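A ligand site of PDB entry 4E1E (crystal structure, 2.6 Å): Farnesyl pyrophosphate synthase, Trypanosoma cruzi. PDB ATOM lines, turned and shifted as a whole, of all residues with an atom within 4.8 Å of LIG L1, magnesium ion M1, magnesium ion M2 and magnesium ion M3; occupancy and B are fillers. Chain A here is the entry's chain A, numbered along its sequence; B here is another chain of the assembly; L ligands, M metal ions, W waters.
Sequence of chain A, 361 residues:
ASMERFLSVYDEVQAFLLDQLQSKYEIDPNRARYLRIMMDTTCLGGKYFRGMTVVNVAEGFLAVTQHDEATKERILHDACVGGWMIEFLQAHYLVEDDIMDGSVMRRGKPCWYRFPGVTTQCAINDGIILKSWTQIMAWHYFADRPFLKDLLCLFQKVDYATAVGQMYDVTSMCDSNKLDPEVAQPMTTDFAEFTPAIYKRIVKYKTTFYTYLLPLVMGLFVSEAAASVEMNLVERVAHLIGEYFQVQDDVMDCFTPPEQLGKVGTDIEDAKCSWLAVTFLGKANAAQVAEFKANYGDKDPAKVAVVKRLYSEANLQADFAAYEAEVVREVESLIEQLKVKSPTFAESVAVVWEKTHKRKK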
ATOM      1  N   TYR A  93      12.093 -15.107   9.395  1.00  0.00           N
ATOM      2  CA  TYR A  93      12.628 -15.068   8.032  1.00  0.00           C
ATOM      3  C   TYR A  93      13.159 -16.425   7.608  1.00  0.00           C
ATOM      4  O   TYR A  93      12.794 -16.912   6.545  1.00  0.00           O
ATOM      5  CB  TYR A  93      13.712 -14.004   7.859  1.00  0.00           C
ATOM      6  CG  TYR A  93      13.211 -12.576   7.999  1.00  0.00           C
ATOM      7  CD1 TYR A  93      11.962 -12.205   7.495  1.00  0.00           C
ATOM      8  CD2 TYR A  93      13.999 -11.603   8.621  1.00  0.00           C
ATOM      9  CE1 TYR A  93      11.495 -10.888   7.622  1.00  0.00           C
ATOM     10  CE2 TYR A  93      13.548 -10.284   8.753  1.00  0.00           C
ATOM     11  CZ  TYR A  93      12.298  -9.924   8.258  1.00  0.00           C
ATOM     12  OH  TYR A  93      11.831  -8.626   8.372  1.00  0.00           O
ATOM     13  N   LEU A  94      13.981 -17.045   8.456  1.00  0.00           N
ATOM     14  CA  LEU A  94      14.612 -18.314   8.126  1.00  0.00           C
ATOM     15  C   LEU A  94      13.596 -19.446   7.856  1.00  0.00           C
ATOM     16  O   LEU A  94      13.712 -20.172   6.856  1.00  0.00           O
ATOM     17  CB  LEU A  94      15.617 -18.716   9.202  1.00  0.00           C
ATOM     18  CG  LEU A  94      16.822 -17.804   9.452  1.00  0.00           C
ATOM     19  CD1 LEU A  94      17.833 -18.571  10.293  1.00  0.00           C
ATOM     20  CD2 LEU A  94      17.467 -17.279   8.164  1.00  0.00           C
ATOM     21  N   GLU A  96      10.559 -19.077   6.828  1.00  0.00           N
ATOM     22  CA  GLU A  96       9.917 -18.766   5.544  1.00  0.00           C
ATOM     23  C   GLU A  96      10.872 -18.876   4.356  1.00  0.00           C
ATOM     24  O   GLU A  96      10.493 -19.353   3.279  1.00  0.00           O
ATOM     25  CB  GLU A  96       9.257 -17.386   5.572  1.00  0.00           C
ATOM     26  CG  GLU A  96       8.311 -17.111   6.759  1.00  0.00           C
ATOM     27  CD  GLU A  96       7.028 -17.938   6.781  1.00  0.00           C
ATOM     28  OE1 GLU A  96       6.735 -18.670   5.795  1.00  0.00           O
ATOM     29  OE2 GLU A  96       6.298 -17.845   7.786  1.00  0.00           O
ATOM     30  N   ASP A  97      12.119 -18.443   4.548  1.00  0.00           N
ATOM     31  CA  ASP A  97      13.144 -18.558   3.514  1.00  0.00           C
ATOM     32  C   ASP A  97      13.436 -20.010   3.151  1.00  0.00           C
ATOM     33  O   ASP A  97      13.567 -20.348   1.961  1.00  0.00           O
ATOM     34  CB  ASP A  97      14.438 -17.906   3.969  1.00  0.00           C
ATOM     35  CG  ASP A  97      15.511 -17.956   2.900  1.00  0.00           C
ATOM     36  OD1 ASP A  97      15.356 -17.242   1.886  1.00  0.00           O
ATOM     37  OD2 ASP A  97      16.505 -18.694   3.075  1.00  0.00           O
ATOM     38  N   ASP A  98      13.527 -20.868   4.159  1.00  0.00           N
ATOM     39  CA  ASP A  98      13.858 -22.257   3.916  1.00  0.00           C
ATOM     40  C   ASP A  98      12.848 -22.935   3.000  1.00  0.00           C
ATOM     41  O   ASP A  98      13.236 -23.627   2.055  1.00  0.00           O
ATOM     42  CB  ASP A  98      14.038 -23.009   5.223  1.00  0.00           C
ATOM     43  CG  ASP A  98      15.362 -22.704   5.886  1.00  0.00           C
ATOM     44  OD1 ASP A  98      16.243 -22.150   5.185  1.00  0.00           O
ATOM     45  OD2 ASP A  98      15.522 -23.009   7.088  1.00  0.00           O
ATOM     46  N   MET A 100      10.947 -21.339   0.929  1.00  0.00           N
ATOM     47  CA  MET A 100      11.095 -20.635  -0.338  1.00  0.00           C
ATOM     48  C   MET A 100      12.321 -21.082  -1.133  1.00  0.00           C
ATOM     49  O   MET A 100      12.318 -21.024  -2.364  1.00  0.00           O
ATOM     50  CB  MET A 100      11.131 -19.125  -0.106  1.00  0.00           C
ATOM     51  CG  MET A 100       9.766 -18.552   0.202  1.00  0.00           C
ATOM     52  SD  MET A 100       9.810 -16.768   0.208  1.00  0.00           S
ATOM     53  CE  MET A 100       9.922 -16.409   1.951  1.00  0.00           C
ATOM     54  N   ASP A 101      13.357 -21.541  -0.431  1.00  0.00           N
ATOM     55  CA  ASP A 101      14.579 -22.020  -1.065  1.00  0.00           C
ATOM     56  C   ASP A 101      14.682 -23.540  -1.125  1.00  0.00           C
ATOM     57  O   ASP A 101      15.689 -24.078  -1.617  1.00  0.00           O
ATOM     58  CB  ASP A 101      15.806 -21.453  -0.353  1.00  0.00           C
ATOM     59  CG  ASP A 101      15.855 -19.952  -0.372  1.00  0.00           C
ATOM     60  OD1 ASP A 101      15.095 -19.318  -1.139  1.00  0.00           O
ATOM     61  OD2 ASP A 101      16.660 -19.376   0.385  1.00  0.00           O
ATOM     62  N   SER A 103      15.237 -25.611   1.246  1.00  0.00           N
ATOM     63  CA  SER A 103      16.412 -26.042   2.016  1.00  0.00           C
ATOM     64  C   SER A 103      16.162 -27.288   2.879  1.00  0.00           C
ATOM     65  O   SER A 103      15.012 -27.643   3.167  1.00  0.00           O
ATOM     66  CB  SER A 103      16.935 -24.895   2.894  1.00  0.00           C
ATOM     67  OG  SER A 103      17.425 -23.827   2.115  1.00  0.00           O
ATOM     68  N   ARG A 106      19.486 -26.475   8.690  1.00  0.00           N
ATOM     69  CA  ARG A 106      19.596 -25.112   9.245  1.00  0.00           C
ATOM     70  C   ARG A 106      20.044 -25.133  10.706  1.00  0.00           C
ATOM     71  O   ARG A 106      19.449 -25.811  11.538  1.00  0.00           O
ATOM     72  CB  ARG A 106      18.266 -24.347   9.097  1.00  0.00           C
ATOM     73  CG  ARG A 106      18.190 -23.026   9.847  1.00  0.00           C
ATOM     74  CD  ARG A 106      18.953 -21.912   9.152  1.00  0.00           C
ATOM     75  NE  ARG A 106      18.187 -21.379   8.040  1.00  0.00           N
ATOM     76  CZ  ARG A 106      18.628 -20.479   7.165  1.00  0.00           C
ATOM     77  NH1 ARG A 106      19.854 -19.982   7.258  1.00  0.00           N
ATOM     78  NH2 ARG A 106      17.832 -20.079   6.177  1.00  0.00           N
ATOM     79  N   THR A 162      13.019  -5.852   4.074  1.00  0.00           N
ATOM     80  CA  THR A 162      13.469  -7.242   3.964  1.00  0.00           C
ATOM     81  C   THR A 162      12.602  -8.044   2.992  1.00  0.00           C
ATOM     82  O   THR A 162      13.121  -8.788   2.160  1.00  0.00           O
ATOM     83  CB  THR A 162      13.485  -7.936   5.341  1.00  0.00           C
ATOM     84  OG1 THR A 162      14.348  -7.200   6.221  1.00  0.00           O
ATOM     85  CG2 THR A 162      13.961  -9.368   5.238  1.00  0.00           C
ATOM     86  N   GLN A 166      13.430  -9.961  -0.532  1.00  0.00           N
ATOM     87  CA  GLN A 166      13.093 -11.354  -0.884  1.00  0.00           C
ATOM     88  C   GLN A 166      12.449 -11.457  -2.242  1.00  0.00           C
ATOM     89  O   GLN A 166      12.763 -12.371  -2.999  1.00  0.00           O
ATOM     90  CB  GLN A 166      12.165 -11.979   0.133  1.00  0.00           C
ATOM     91  CG  GLN A 166      12.871 -12.712   1.225  1.00  0.00           C
ATOM     92  CD  GLN A 166      13.624 -13.934   0.743  1.00  0.00           C
ATOM     93  OE1 GLN A 166      14.832 -13.862   0.562  1.00  0.00           O
ATOM     94  NE2 GLN A 166      12.926 -15.039   0.554  1.00  0.00           N
ATOM     95  N   ASP A 169      14.947 -11.277  -4.694  1.00  0.00           N
ATOM     96  CA  ASP A 169      15.805 -12.451  -4.555  1.00  0.00           C
ATOM     97  C   ASP A 169      15.226 -13.716  -5.182  1.00  0.00           C
ATOM     98  O   ASP A 169      15.959 -14.491  -5.806  1.00  0.00           O
ATOM     99  CB  ASP A 169      16.114 -12.690  -3.073  1.00  0.00           C
ATOM    100  CG  ASP A 169      17.059 -13.845  -2.852  1.00  0.00           C
ATOM    101  OD1 ASP A 169      18.277 -13.605  -2.823  1.00  0.00           O
ATOM    102  OD2 ASP A 169      16.596 -14.991  -2.696  1.00  0.00           O
ATOM    103  N   LYS A 206      17.240  -7.339   1.227  1.00  0.00           N
ATOM    104  CA  LYS A 206      17.042  -8.670   1.839  1.00  0.00           C
ATOM    105  C   LYS A 206      17.942  -8.969   3.048  1.00  0.00           C
ATOM    106  O   LYS A 206      17.645  -9.886   3.795  1.00  0.00           O
ATOM    107  CB  LYS A 206      17.127  -9.813   0.815  1.00  0.00           C
ATOM    108  CG  LYS A 206      18.530 -10.335   0.560  1.00  0.00           C
ATOM    109  CD  LYS A 206      18.535 -11.747   0.023  1.00  0.00           C
ATOM    110  CE  LYS A 206      19.928 -12.138  -0.417  1.00  0.00           C
ATOM    111  NZ  LYS A 206      20.009 -13.562  -0.798  1.00  0.00           N
ATOM    112  N   TYR A 210      17.802  -5.459   8.159  1.00  0.00           N
ATOM    113  CA  TYR A 210      17.499  -6.229   9.362  1.00  0.00           C
ATOM    114  C   TYR A 210      18.702  -6.806  10.107  1.00  0.00           C
ATOM    115  O   TYR A 210      18.623  -7.105  11.292  1.00  0.00           O
ATOM    116  CB  TYR A 210      16.405  -7.281   9.079  1.00  0.00           C
ATOM    117  CG  TYR A 210      16.864  -8.676   8.769  1.00  0.00           C
ATOM    118  CD1 TYR A 210      17.013  -9.622   9.777  1.00  0.00           C
ATOM    119  CD2 TYR A 210      17.119  -9.074   7.448  1.00  0.00           C
ATOM    120  CE1 TYR A 210      17.423 -10.920   9.506  1.00  0.00           C
ATOM    121  CE2 TYR A 210      17.524 -10.382   7.162  1.00  0.00           C
ATOM    122  CZ  TYR A 210      17.673 -11.292   8.196  1.00  0.00           C
ATOM    123  OH  TYR A 210      18.071 -12.574   7.957  1.00  0.00           O
ATOM    124  N   GLN A 246      26.612 -10.556   3.280  1.00  0.00           N
ATOM    125  CA  GLN A 246      25.864 -11.355   2.313  1.00  0.00           C
ATOM    126  C   GLN A 246      26.792 -11.945   1.269  1.00  0.00           C
ATOM    127  O   GLN A 246      26.628 -13.123   0.886  1.00  0.00           O
ATOM    128  CB  GLN A 246      24.753 -10.527   1.655  1.00  0.00           C
ATOM    129  CG  GLN A 246      23.841 -11.339   0.743  1.00  0.00           C
ATOM    130  CD  GLN A 246      23.145 -12.489   1.451  1.00  0.00           C
ATOM    131  OE1 GLN A 246      22.598 -12.326   2.543  1.00  0.00           O
ATOM    132  NE2 GLN A 246      23.171 -13.675   0.841  1.00  0.00           N
ATOM    133  N   ASP A 249      28.204 -14.852   2.924  1.00  0.00           N
ATOM    134  CA  ASP A 249      27.199 -15.928   2.976  1.00  0.00           C
ATOM    135  C   ASP A 249      27.125 -16.643   1.635  1.00  0.00           C
ATOM    136  O   ASP A 249      26.998 -17.872   1.588  1.00  0.00           O
ATOM    137  CB  ASP A 249      25.830 -15.340   3.364  1.00  0.00           C
ATOM    138  CG  ASP A 249      24.675 -16.353   3.265  1.00  0.00           C
ATOM    139  OD1 ASP A 249      24.501 -17.194   4.168  1.00  0.00           O
ATOM    140  OD2 ASP A 249      23.899 -16.264   2.291  1.00  0.00           O
ATOM    141  N   ASP A 250      27.234 -15.871   0.550  1.00  0.00           N
ATOM    142  CA  ASP A 250      27.208 -16.390  -0.826  1.00  0.00           C
ATOM    143  C   ASP A 250      28.390 -17.302  -1.130  1.00  0.00           C
ATOM    144  O   ASP A 250      28.200 -18.368  -1.717  1.00  0.00           O
ATOM    145  CB  ASP A 250      27.162 -15.233  -1.837  1.00  0.00           C
ATOM    146  CG  ASP A 250      25.774 -14.620  -1.988  1.00  0.00           C
ATOM    147  OD1 ASP A 250      24.825 -15.023  -1.275  1.00  0.00           O
ATOM    148  OD2 ASP A 250      25.627 -13.713  -2.832  1.00  0.00           O
ATOM    149  N   ASP A 253      28.058 -20.611   0.681  1.00  0.00           N
ATOM    150  CA  ASP A 253      27.024 -21.463   0.078  1.00  0.00           C
ATOM    151  C   ASP A 253      27.642 -22.388  -0.969  1.00  0.00           C
ATOM    152  O   ASP A 253      27.169 -23.501  -1.183  1.00  0.00           O
ATOM    153  CB  ASP A 253      25.911 -20.628  -0.558  1.00  0.00           C
ATOM    154  CG  ASP A 253      24.597 -21.400  -0.674  1.00  0.00           C
ATOM    155  OD1 ASP A 253      23.865 -21.505   0.338  1.00  0.00           O
ATOM    156  OD2 ASP A 253      24.292 -21.886  -1.784  1.00  0.00           O
ATOM    157  N   LYS A 263      24.557 -25.402   7.076  1.00  0.00           N
ATOM    158  CA  LYS A 263      23.401 -25.565   6.207  1.00  0.00           C
ATOM    159  C   LYS A 263      23.937 -26.071   4.870  1.00  0.00           C
ATOM    160  O   LYS A 263      25.149 -26.007   4.630  1.00  0.00           O
ATOM    161  CB  LYS A 263      22.596 -24.256   6.071  1.00  0.00           C
ATOM    162  CG  LYS A 263      23.366 -23.101   5.434  1.00  0.00           C
ATOM    163  CD  LYS A 263      22.949 -21.737   5.989  1.00  0.00           C
ATOM    164  CE  LYS A 263      23.459 -20.605   5.096  1.00  0.00           C
ATOM    165  NZ  LYS A 263      23.297 -19.239   5.659  1.00  0.00           N
ATOM    166  N   ASP A 267      22.158 -22.297  -3.782  1.00  0.00           N
ATOM    167  CA  ASP A 267      22.267 -21.114  -4.664  1.00  0.00           C
ATOM    168  C   ASP A 267      22.435 -21.467  -6.134  1.00  0.00           C
ATOM    169  O   ASP A 267      21.828 -20.817  -6.992  1.00  0.00           O
ATOM    170  CB  ASP A 267      23.374 -20.153  -4.199  1.00  0.00           C
ATOM    171  CG  ASP A 267      22.964 -19.307  -2.985  1.00  0.00           C
ATOM    172  OD1 ASP A 267      21.778 -19.381  -2.584  1.00  0.00           O
ATOM    173  OD2 ASP A 267      23.813 -18.579  -2.434  1.00  0.00           O
ATOM    174  N   LYS A 272      20.254 -18.808  -8.012  1.00  0.00           N
ATOM    175  CA  LYS A 272      20.366 -17.556  -7.271  1.00  0.00           C
ATOM    176  C   LYS A 272      21.382 -16.589  -7.858  1.00  0.00           C
ATOM    177  O   LYS A 272      22.492 -16.978  -8.210  1.00  0.00           O
ATOM    178  CB  LYS A 272      20.654 -17.796  -5.781  1.00  0.00           C
ATOM    179  CG  LYS A 272      19.437 -18.280  -4.981  1.00  0.00           C
ATOM    180  CD  LYS A 272      18.344 -17.205  -4.944  1.00  0.00           C
ATOM    181  CE  LYS A 272      16.959 -17.809  -5.097  1.00  0.00           C
ATOM    182  NZ  LYS A 272      16.638 -18.792  -4.033  1.00  0.00           N
ATOM    183  N   ASN B 125       5.945 -15.103   0.306  1.00  0.00           N
ATOM    184  CA  ASN B 125       6.459 -13.739   0.438  1.00  0.00           C
ATOM    185  C   ASN B 125       5.409 -12.682   0.108  1.00  0.00           C
ATOM    186  O   ASN B 125       5.329 -11.655   0.791  1.00  0.00           O
ATOM    187  CB  ASN B 125       7.737 -13.524  -0.392  1.00  0.00           C
ATOM    188  CG  ASN B 125       8.608 -12.395   0.158  1.00  0.00           C
ATOM    189  OD1 ASN B 125       9.201 -12.516   1.245  1.00  0.00           O
ATOM    190  ND2 ASN B 125       8.699 -11.307  -0.592  1.00  0.00           N
ATOM    191  N   ILE B 128       3.542 -12.099   3.127  1.00  0.00           N
ATOM    192  CA  ILE B 128       4.314 -11.301   4.074  1.00  0.00           C
ATOM    193  C   ILE B 128       4.231  -9.817   3.699  1.00  0.00           C
ATOM    194  O   ILE B 128       4.089  -8.967   4.562  1.00  0.00           O
ATOM    195  CB  ILE B 128       5.785 -11.753   4.137  1.00  0.00           C
ATOM    196  CG1 ILE B 128       5.881 -13.146   4.785  1.00  0.00           C
ATOM    197  CG2 ILE B 128       6.639 -10.712   4.865  1.00  0.00           C
ATOM    198  CD1 ILE B 128       7.249 -13.800   4.669  1.00  0.00           C
HETATM  199  O1  LIG L   1      19.383 -19.482   3.384  1.00  0.00           O
HETATM  200  P1  LIG L   1      20.243 -18.316   3.813  1.00  0.00           P
HETATM  201  O2  LIG L   1      21.531 -18.186   3.050  1.00  0.00           O
HETATM  202  O3  LIG L   1      20.399 -18.231   5.309  1.00  0.00           O
HETATM  203  C1  LIG L   1      19.199 -16.892   3.360  1.00  0.00           C
HETATM  204  P2  LIG L   1      19.618 -16.413   1.657  1.00  0.00           P
HETATM  205  O4  LIG L   1      21.108 -16.389   1.544  1.00  0.00           O
HETATM  206  O5  LIG L   1      18.982 -17.551   0.889  1.00  0.00           O
HETATM  207  O6  LIG L   1      19.024 -15.050   1.409  1.00  0.00           O
HETATM  208  C2  LIG L   1      19.348 -15.765   4.386  1.00  0.00           C
HETATM  209  N1  LIG L   1      18.668 -14.513   3.991  1.00  0.00           N
HETATM  210  C3  LIG L   1      17.332 -14.416   4.583  1.00  0.00           C
HETATM  211  C4  LIG L   1      16.390 -13.815   3.551  1.00  0.00           C
HETATM  212  C5  LIG L   1      15.291 -12.974   4.187  1.00  0.00           C
HETATM  213  C6  LIG L   1      14.036 -13.819   4.275  1.00  0.00           C
HETATM  214  C7  LIG L   1      12.756 -12.988   4.229  1.00  0.00           C
HETATM  215  C8  LIG L   1      11.561 -13.900   4.165  1.00  0.00           C
HETATM  216  C1  LG2 L   2      23.110 -16.437   7.466  1.00  0.00           C
HETATM  217  O1  LG2 L   2      23.563 -16.515   8.838  1.00  0.00           O
HETATM  218  C2  LG2 L   2      21.691 -15.876   7.311  1.00  0.00           C
HETATM  219  C3  LG2 L   2      21.663 -14.656   6.390  1.00  0.00           C
HETATM  220  C4  LG2 L   2      20.743 -13.729   6.552  1.00  0.00           C
HETATM  221  C5  LG2 L   2      22.648 -14.479   5.264  1.00  0.00           C
HETATM  222  P1  LG2 L   2      22.943 -15.588   9.998  1.00  0.00           P
HETATM  223  O2  LG2 L   2      22.023 -14.621   9.316  1.00  0.00           O
HETATM  224  O3  LG2 L   2      24.042 -15.043  10.870  1.00  0.00           O
HETATM  225  O4  LG2 L   2      22.013 -16.617  10.834  1.00  0.00           O
HETATM  226  P2  LG2 L   2      22.170 -17.131  12.354  1.00  0.00           P
HETATM  227  O5  LG2 L   2      22.696 -18.537  12.190  1.00  0.00           O
HETATM  228  O6  LG2 L   2      20.753 -17.098  12.842  1.00  0.00           O
HETATM  229  O7  LG2 L   2      23.117 -16.182  13.073  1.00  0.00           O
HETATM  230 MG    MG M   1      22.758 -17.749   1.096  1.00  0.00          MG
HETATM  231 MG    MG M   2      18.326 -19.649   1.803  1.00  0.00          MG
HETATM  232 MG    MG M   3      16.900 -17.187   0.225  1.00  0.00          MG
HETATM  233  O   HOH W   1      18.083 -16.833  -1.719  1.00  0.00           O
HETATM  234  O   HOH W   2      24.124 -19.251   2.164  1.00  0.00           O
HETATM  235  O   HOH W   3      15.138 -16.758  -1.011  1.00  0.00           O
HETATM  236  O   HOH W   4      16.840 -15.015   0.173  1.00  0.00           O
HETATM  237  O   HOH W   5      17.137 -21.183   2.908  1.00  0.00           O
HETATM  238  O   HOH W   6      21.659 -19.345   0.412  1.00  0.00           O
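NH1 of Arg 106 is in salt-bridge range of O3 of LIG L1 (2.7 Å). The side-chain amino group (NZ) of Lys 206 lies within salt-bridge range of an oxygen (O6) of LIG L1 (2.8 Å). The side-chain amino group (NZ) of Lys 263 lies within salt-bridge range of an oxygen (O3) of LIG L1 (3.1 Å). NE2 of Gln 246 sits close to O4 of LIG L1 (3.5 Å).
The side-chain carboxylate (OD1) of Asp 101 lies within salt-bridge range of the side-chain amino group (NZ) of Lys 272 (3.3 Å). The side-chain amino group of Lys 263 lies within salt-bridge range of the side-chain carboxylate of Asp 249, 2.8 Å away. NE2 of Gln 246 lies close to OD2 of Asp 249, 3.1 Å away. OD2 of Asp 97 sits close to NH2 of Arg 106, 3.6 Å away. The side-chain carboxylate (OD1) of Asp 169 is in salt-bridge range of the side-chain amino group (NZ) of Lys 206, 2.7 Å away. NE2 of Gln 166 is in hydrogen-bond range of SD of Met 100, at 3.6 Å. The side-chain amide nitrogen (NE2) of Gln 246 lies within hydrogen-bond range of the side-chain carboxylate (OD1) of Asp 250 (3.0 Å). O of Asp 267 sits at hydrogen-bond distance from N of Lys 272 (2.7 Å).
Merely in contact with LIG L1: Gln 166 (3.0 Å), Tyr 93 (3.5 Å), Met 100 (3.7 Å), Tyr 210 (3.9 Å) and Thr 162 (3.9 Å). Hydrophobic or aromatic side chains within 4 Å of LIG L1: Tyr 93 and Met 100. Of the 23 residues printed, 12 come within 4 Å of LIG L1. The nearest printed residue that does not touch LIG L1 is Asn 125 of chain B (4.001 Å).
Residues that only touch magnesium ion M1: Asp 267 and Asp 253. The nearest printed residue that does not touch magnesium ion M1 is Gln 246 (4.1 Å).
Of the 23 residues printed, 2 come within 4 Å of magnesium ion M2. The nearest printed residue that does not touch magnesium ion M2 is Ser 103 (4.3 Å).
Residues that only touch magnesium ion M3: Gln 166 and Asp 169. The nearest printed residue that does not touch magnesium ion M3 is Lys 272 (4.6 Å).
Water W6 is bound to magnesium ion M1 (2.1 Å). O4 of LIG L1 is bound to magnesium ion M1, 2.2 Å away. OD2 of Asp 249 is bound to magnesium ion M1, 2.2 Å away. Magnesium ion M1 is bound by water W2 (2.3 Å). Magnesium ion M1 is bound by O2 of LIG L1 (2.3 Å). Magnesium ion M1 has five donor atoms within binding distance.
Magnesium ion M2 is bound by O1 of LIG L1 (1.9 Å). The side-chain carboxylate (OD2) of Asp 101 binds magnesium ion M2. Magnesium ion M2 is bound by water W5, at 2.2 Å. O5 of LIG L1 is bound to magnesium ion M2, at 2.4 Å. Magnesium ion M2 is bound by OD2 of Asp 97.
Magnesium ion M3 is bound by water W4 (2.2 Å), water W3 (2.2 Å), the side-chain carboxylate (OD2) of Asp 101 (2.2 Å), an oxygen (O5) of LIG L1 (2.2 Å), the side-chain carboxylate (OD1) of Asp 97 (2.3 Å) and water W1 (2.3 Å).
Water W6 lies within hydrogen-bond range of OD1 of Asp 267 (3.0 Å) and OD1 of Asp 253 (3.1 Å). Water W2 lies within hydrogen-bond range of the side-chain carboxylate (OD1) of Asp 249 (2.9 Å) and the side-chain carboxylate (OD1) of Asp 253 (2.9 Å). Water W5 lies within hydrogen-bond range of OD1 of Asp 98 (2.6 Å) and OG of Ser 103 (2.8 Å). Water W3 lies within hydrogen-bond range of OD1 of Asp 101 (2.6 Å), OD2 of Asp 169 (2.8 Å) and NE2 of Gln 166 (3.2 Å). Water W4 bridges an oxygen (O6) of LIG L1 (2.5 Å) and the side-chain carboxylate (OD2) of Asp 169 (2.9 Å). Water W1 lies within hydrogen-bond range of OD2 of Asp 169 (2.6 Å) and NZ of Lys 272 (3.4 Å).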
